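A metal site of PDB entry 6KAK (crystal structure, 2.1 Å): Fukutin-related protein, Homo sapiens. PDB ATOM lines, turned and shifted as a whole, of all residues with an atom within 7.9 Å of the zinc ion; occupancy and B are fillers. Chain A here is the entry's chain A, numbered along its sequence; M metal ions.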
ATOM      1  N   ARG A 235      -9.611  34.476  -8.532  1.00  0.00           N
ATOM      2  CA  ARG A 235      -9.650  33.155  -9.133  1.00  0.00           C
ATOM      3  C   ARG A 235     -10.626  33.049 -10.297  1.00  0.00           C
ATOM      4  O   ARG A 235     -10.510  32.105 -11.097  1.00  0.00           O
ATOM      5  CB  ARG A 235     -10.031  32.105  -8.075  1.00  0.00           C
ATOM      6  CG  ARG A 235      -9.060  31.996  -6.932  1.00  0.00           C
ATOM      7  CD  ARG A 235      -7.979  30.992  -7.241  1.00  0.00           C
ATOM      8  NE  ARG A 235      -7.201  30.647  -6.051  1.00  0.00           N
ATOM      9  CZ  ARG A 235      -6.218  31.398  -5.568  1.00  0.00           C
ATOM     10  NH1 ARG A 235      -5.878  32.524  -6.176  1.00  0.00           N
ATOM     11  NH2 ARG A 235      -5.570  31.010  -4.479  1.00  0.00           N
ATOM     12  N   TRP A 246     -11.073  31.312 -15.593  1.00  0.00           N
ATOM     13  CA  TRP A 246     -10.622  30.695 -14.353  1.00  0.00           C
ATOM     14  C   TRP A 246      -9.116  30.866 -14.171  1.00  0.00           C
ATOM     15  O   TRP A 246      -8.347  30.788 -15.142  1.00  0.00           O
ATOM     16  CB  TRP A 246     -10.967  29.201 -14.330  1.00  0.00           C
ATOM     17  CG  TRP A 246     -12.445  28.926 -14.281  1.00  0.00           C
ATOM     18  CD1 TRP A 246     -13.251  28.572 -15.324  1.00  0.00           C
ATOM     19  CD2 TRP A 246     -13.284  28.996 -13.128  1.00  0.00           C
ATOM     20  NE1 TRP A 246     -14.542  28.405 -14.888  1.00  0.00           N
ATOM     21  CE2 TRP A 246     -14.592  28.655 -13.546  1.00  0.00           C
ATOM     22  CE3 TRP A 246     -13.069  29.292 -11.777  1.00  0.00           C
ATOM     23  CZ2 TRP A 246     -15.671  28.622 -12.667  1.00  0.00           C
ATOM     24  CZ3 TRP A 246     -14.143  29.253 -10.905  1.00  0.00           C
ATOM     25  CH2 TRP A 246     -15.430  28.918 -11.354  1.00  0.00           C
ATOM     26  N   PHE A 247      -8.704  31.079 -12.935  1.00  0.00           N
ATOM     27  CA  PHE A 247      -7.301  31.297 -12.591  1.00  0.00           C
ATOM     28  C   PHE A 247      -6.935  30.578 -11.296  1.00  0.00           C
ATOM     29  O   PHE A 247      -6.132  31.066 -10.501  1.00  0.00           O
ATOM     30  CB  PHE A 247      -7.004  32.798 -12.484  1.00  0.00           C
ATOM     31  CG  PHE A 247      -7.223  33.544 -13.766  1.00  0.00           C
ATOM     32  CD1 PHE A 247      -6.215  33.633 -14.720  1.00  0.00           C
ATOM     33  CD2 PHE A 247      -8.436  34.169 -14.024  1.00  0.00           C
ATOM     34  CE1 PHE A 247      -6.415  34.318 -15.906  1.00  0.00           C
ATOM     35  CE2 PHE A 247      -8.644  34.850 -15.213  1.00  0.00           C
ATOM     36  CZ  PHE A 247      -7.630  34.934 -16.144  1.00  0.00           C
ATOM     37  N   GLY A 248      -7.522  29.401 -11.086  1.00  0.00           N
ATOM     38  CA  GLY A 248      -7.336  28.643  -9.858  1.00  0.00           C
ATOM     39  C   GLY A 248      -6.892  27.218 -10.128  1.00  0.00           C
ATOM     40  O   GLY A 248      -6.049  26.957 -10.990  1.00  0.00           O
ATOM     41  N   CYS A 249      -7.463  26.291  -9.368  1.00  0.00           N
ATOM     42  CA  CYS A 249      -7.129  24.879  -9.470  1.00  0.00           C
ATOM     43  C   CYS A 249      -8.035  24.178 -10.480  1.00  0.00           C
ATOM     44  O   CYS A 249      -9.063  24.711 -10.910  1.00  0.00           O
ATOM     45  CB  CYS A 249      -7.234  24.210  -8.098  1.00  0.00           C
ATOM     46  SG  CYS A 249      -8.912  23.994  -7.487  1.00  0.00           S
ATOM     47  N   ASN A 250      -7.631  22.972 -10.873  1.00  0.00           N
ATOM     48  CA  ASN A 250      -8.400  22.195 -11.834  1.00  0.00           C
ATOM     49  C   ASN A 250      -8.033  20.718 -11.673  1.00  0.00           C
ATOM     50  O   ASN A 250      -7.275  20.336 -10.777  1.00  0.00           O
ATOM     51  CB  ASN A 250      -8.163  22.681 -13.267  1.00  0.00           C
ATOM     52  CG  ASN A 250      -6.690  22.620 -13.673  1.00  0.00           C
ATOM     53  OD1 ASN A 250      -6.061  21.554 -13.633  1.00  0.00           O
ATOM     54  ND2 ASN A 250      -6.140  23.752 -14.086  1.00  0.00           N
ATOM     55  N   THR A 253      -4.302  19.916 -11.319  1.00  0.00           N
ATOM     56  CA  THR A 253      -3.482  20.581 -10.316  1.00  0.00           C
ATOM     57  C   THR A 253      -3.865  20.087  -8.920  1.00  0.00           C
ATOM     58  O   THR A 253      -4.847  19.363  -8.737  1.00  0.00           O
ATOM     59  CB  THR A 253      -3.650  22.103 -10.373  1.00  0.00           C
ATOM     60  OG1 THR A 253      -4.918  22.481  -9.825  1.00  0.00           O
ATOM     61  CG2 THR A 253      -3.559  22.603 -11.804  1.00  0.00           C
ATOM     62  N   THR A 254      -3.061  20.492  -7.942  1.00  0.00           N
ATOM     63  CA  THR A 254      -3.466  20.408  -6.553  1.00  0.00           C
ATOM     64  C   THR A 254      -4.610  21.392  -6.301  1.00  0.00           C
ATOM     65  O   THR A 254      -4.794  22.373  -7.040  1.00  0.00           O
ATOM     66  CB  THR A 254      -2.297  20.715  -5.620  1.00  0.00           C
ATOM     67  OG1 THR A 254      -2.702  20.505  -4.257  1.00  0.00           O
ATOM     68  CG2 THR A 254      -1.829  22.153  -5.787  1.00  0.00           C
ATOM     69  N   ARG A 255      -5.388  21.127  -5.265  1.00  0.00           N
ATOM     70  CA  ARG A 255      -6.412  22.084  -4.884  1.00  0.00           C
ATOM     71  C   ARG A 255      -5.753  23.321  -4.277  1.00  0.00           C
ATOM     72  O   ARG A 255      -4.588  23.312  -3.867  1.00  0.00           O
ATOM     73  CB  ARG A 255      -7.416  21.470  -3.913  1.00  0.00           C
ATOM     74  CG  ARG A 255      -6.884  21.217  -2.508  1.00  0.00           C
ATOM     75  CD  ARG A 255      -7.872  20.407  -1.682  1.00  0.00           C
ATOM     76  NE  ARG A 255      -7.355  20.135  -0.343  1.00  0.00           N
ATOM     77  CZ  ARG A 255      -7.942  19.341   0.549  1.00  0.00           C
ATOM     78  NH1 ARG A 255      -9.082  18.736   0.248  1.00  0.00           N
ATOM     79  NH2 ARG A 255      -7.392  19.158   1.735  1.00  0.00           N
ATOM     80  N   CYS A 256      -6.521  24.413  -4.221  1.00  0.00           N
ATOM     81  CA  CYS A 256      -5.952  25.719  -3.890  1.00  0.00           C
ATOM     82  C   CYS A 256      -5.338  25.730  -2.487  1.00  0.00           C
ATOM     83  O   CYS A 256      -4.211  26.200  -2.297  1.00  0.00           O
ATOM     84  CB  CYS A 256      -7.003  26.816  -4.030  1.00  0.00           C
ATOM     85  SG  CYS A 256      -7.407  27.226  -5.722  1.00  0.00           S
ATOM     86  N   PHE A 257      -6.062  25.217  -1.492  1.00  0.00           N
ATOM     87  CA  PHE A 257      -5.627  25.329  -0.115  1.00  0.00           C
ATOM     88  C   PHE A 257      -4.805  24.133   0.357  1.00  0.00           C
ATOM     89  O   PHE A 257      -4.386  24.117   1.520  1.00  0.00           O
ATOM     90  CB  PHE A 257      -6.821  25.567   0.818  1.00  0.00           C
ATOM     91  CG  PHE A 257      -7.964  24.604   0.625  1.00  0.00           C
ATOM     92  CD1 PHE A 257      -8.954  24.849  -0.318  1.00  0.00           C
ATOM     93  CD2 PHE A 257      -8.062  23.469   1.418  1.00  0.00           C
ATOM     94  CE1 PHE A 257     -10.008  23.969  -0.481  1.00  0.00           C
ATOM     95  CE2 PHE A 257      -9.116  22.589   1.256  1.00  0.00           C
ATOM     96  CZ  PHE A 257     -10.079  22.833   0.304  1.00  0.00           C
ATOM     97  N   THR A 274     -14.294  29.943   0.508  1.00  0.00           N
ATOM     98  CA  THR A 274     -13.729  28.914  -0.359  1.00  0.00           C
ATOM     99  C   THR A 274     -13.501  29.473  -1.766  1.00  0.00           C
ATOM    100  O   THR A 274     -14.377  30.162  -2.313  1.00  0.00           O
ATOM    101  CB  THR A 274     -14.641  27.694  -0.425  1.00  0.00           C
ATOM    102  OG1 THR A 274     -14.945  27.253   0.903  1.00  0.00           O
ATOM    103  CG2 THR A 274     -13.973  26.559  -1.176  1.00  0.00           C
ATOM    104  N   PRO A 275     -12.349  29.208  -2.373  1.00  0.00           N
ATOM    105  CA  PRO A 275     -12.116  29.625  -3.762  1.00  0.00           C
ATOM    106  C   PRO A 275     -13.186  29.082  -4.687  1.00  0.00           C
ATOM    107  O   PRO A 275     -13.645  27.942  -4.527  1.00  0.00           O
ATOM    108  CB  PRO A 275     -10.738  29.018  -4.075  1.00  0.00           C
ATOM    109  CG  PRO A 275     -10.053  29.038  -2.756  1.00  0.00           C
ATOM    110  CD  PRO A 275     -11.120  28.676  -1.752  1.00  0.00           C
ATOM    111  N   PRO A 276     -13.595  29.871  -5.682  1.00  0.00           N
ATOM    112  CA  PRO A 276     -14.702  29.441  -6.557  1.00  0.00           C
ATOM    113  C   PRO A 276     -14.339  28.289  -7.476  1.00  0.00           C
ATOM    114  O   PRO A 276     -15.234  27.572  -7.923  1.00  0.00           O
ATOM    115  CB  PRO A 276     -15.014  30.710  -7.360  1.00  0.00           C
ATOM    116  CG  PRO A 276     -13.698  31.435  -7.400  1.00  0.00           C
ATOM    117  CD  PRO A 276     -13.116  31.225  -6.033  1.00  0.00           C
ATOM    118  N   CYS A 277     -13.049  28.096  -7.775  1.00  0.00           N
ATOM    119  CA  CYS A 277     -12.619  26.919  -8.519  1.00  0.00           C
ATOM    120  C   CYS A 277     -12.733  25.662  -7.679  1.00  0.00           C
ATOM    121  O   CYS A 277     -13.049  24.592  -8.197  1.00  0.00           O
ATOM    122  CB  CYS A 277     -11.183  27.106  -8.997  1.00  0.00           C
ATOM    123  SG  CYS A 277     -10.135  27.779  -7.689  1.00  0.00           S
ATOM    124  N   CYS A 278     -12.469  25.771  -6.375  1.00  0.00           N
ATOM    125  CA  CYS A 278     -12.648  24.636  -5.483  1.00  0.00           C
ATOM    126  C   CYS A 278     -14.121  24.271  -5.354  1.00  0.00           C
ATOM    127  O   CYS A 278     -14.473  23.092  -5.345  1.00  0.00           O
ATOM    128  CB  CYS A 278     -12.047  24.936  -4.108  1.00  0.00           C
ATOM    129  SG  CYS A 278     -10.275  25.311  -4.138  1.00  0.00           S
ATOM    130  N   LEU A 279     -14.986  25.278  -5.235  1.00  0.00           N
ATOM    131  CA  LEU A 279     -16.419  25.016  -5.164  1.00  0.00           C
ATOM    132  C   LEU A 279     -16.923  24.421  -6.475  1.00  0.00           C
ATOM    133  O   LEU A 279     -17.770  23.523  -6.470  1.00  0.00           O
ATOM    134  CB  LEU A 279     -17.178  26.301  -4.831  1.00  0.00           C
ATOM    135  CG  LEU A 279     -17.014  26.844  -3.407  1.00  0.00           C
ATOM    136  CD1 LEU A 279     -17.641  28.226  -3.289  1.00  0.00           C
ATOM    137  CD2 LEU A 279     -17.618  25.899  -2.393  1.00  0.00           C
ATOM    138  N   ARG A 280     -16.411  24.914  -7.601  1.00  0.00           N
ATOM    139  CA  ARG A 280     -16.812  24.362  -8.900  1.00  0.00           C
ATOM    140  C   ARG A 280     -16.463  22.885  -8.989  1.00  0.00           C
ATOM    141  O   ARG A 280     -17.275  22.067  -9.434  1.00  0.00           O
ATOM    142  CB  ARG A 280     -16.149  25.146 -10.028  1.00  0.00           C
ATOM    143  CG  ARG A 280     -16.656  24.784 -11.420  1.00  0.00           C
ATOM    144  CD  ARG A 280     -15.554  24.936 -12.464  1.00  0.00           C
ATOM    145  NE  ARG A 280     -14.413  24.067 -12.197  1.00  0.00           N
ATOM    146  CZ  ARG A 280     -14.393  22.760 -12.447  1.00  0.00           C
ATOM    147  NH1 ARG A 280     -15.459  22.159 -12.965  1.00  0.00           N
ATOM    148  NH2 ARG A 280     -13.310  22.050 -12.164  1.00  0.00           N
ATOM    149  N   ALA A 281     -15.250  22.526  -8.567  1.00  0.00           N
ATOM    150  CA  ALA A 281     -14.838  21.126  -8.610  1.00  0.00           C
ATOM    151  C   ALA A 281     -15.630  20.277  -7.624  1.00  0.00           C
ATOM    152  O   ALA A 281     -15.897  19.096  -7.891  1.00  0.00           O
ATOM    153  CB  ALA A 281     -13.345  21.004  -8.317  1.00  0.00           C
ATOM    154  N   ASN A 371      -5.935  16.572  -7.410  1.00  0.00           N
ATOM    155  CA  ASN A 371      -6.837  17.508  -6.750  1.00  0.00           C
ATOM    156  C   ASN A 371      -7.710  16.753  -5.759  1.00  0.00           C
ATOM    157  O   ASN A 371      -8.593  15.976  -6.155  1.00  0.00           O
ATOM    158  CB  ASN A 371      -7.697  18.245  -7.780  1.00  0.00           C
ATOM    159  CG  ASN A 371      -8.399  19.455  -7.202  1.00  0.00           C
ATOM    160  OD1 ASN A 371      -8.916  19.412  -6.086  1.00  0.00           O
ATOM    161  ND2 ASN A 371      -8.438  20.543  -7.972  1.00  0.00           N
ATOM    162  N   LEU A 373     -10.083  17.644  -3.571  1.00  0.00           N
ATOM    163  CA  LEU A 373     -11.424  18.034  -3.165  1.00  0.00           C
ATOM    164  C   LEU A 373     -12.336  16.815  -3.231  1.00  0.00           C
ATOM    165  O   LEU A 373     -12.310  16.068  -4.215  1.00  0.00           O
ATOM    166  CB  LEU A 373     -11.941  19.151  -4.072  1.00  0.00           C
ATOM    167  CG  LEU A 373     -11.171  20.469  -3.933  1.00  0.00           C
ATOM    168  CD1 LEU A 373     -11.272  21.312  -5.190  1.00  0.00           C
ATOM    169  CD2 LEU A 373     -11.664  21.241  -2.712  1.00  0.00           C
HETATM  170 ZN    ZN M   1      -9.428  26.023  -6.235  1.00  0.00          ZN
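Pro 275 touches the zinc ion.
Five residues have an atom within 4 Å of the zinc ion: Cys 249, Cys 256, Pro 275, Cys 277 and Cys 278.
ND2 of Asn 371 sits close to SG of Cys 249 (3.5 Å).
NE of Arg 235 sits close to SG of Cys 256, 3.4 Å away.
The zinc ion is bound by the side-chain sulfur of Cys 278 (2.4 Å), the side-chain sulfur of Cys 277 (2.4 Å), the side-chain sulfur of Cys 256 (2.4 Å) and the side-chain sulfur of Cys 249 (2.4 Å).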
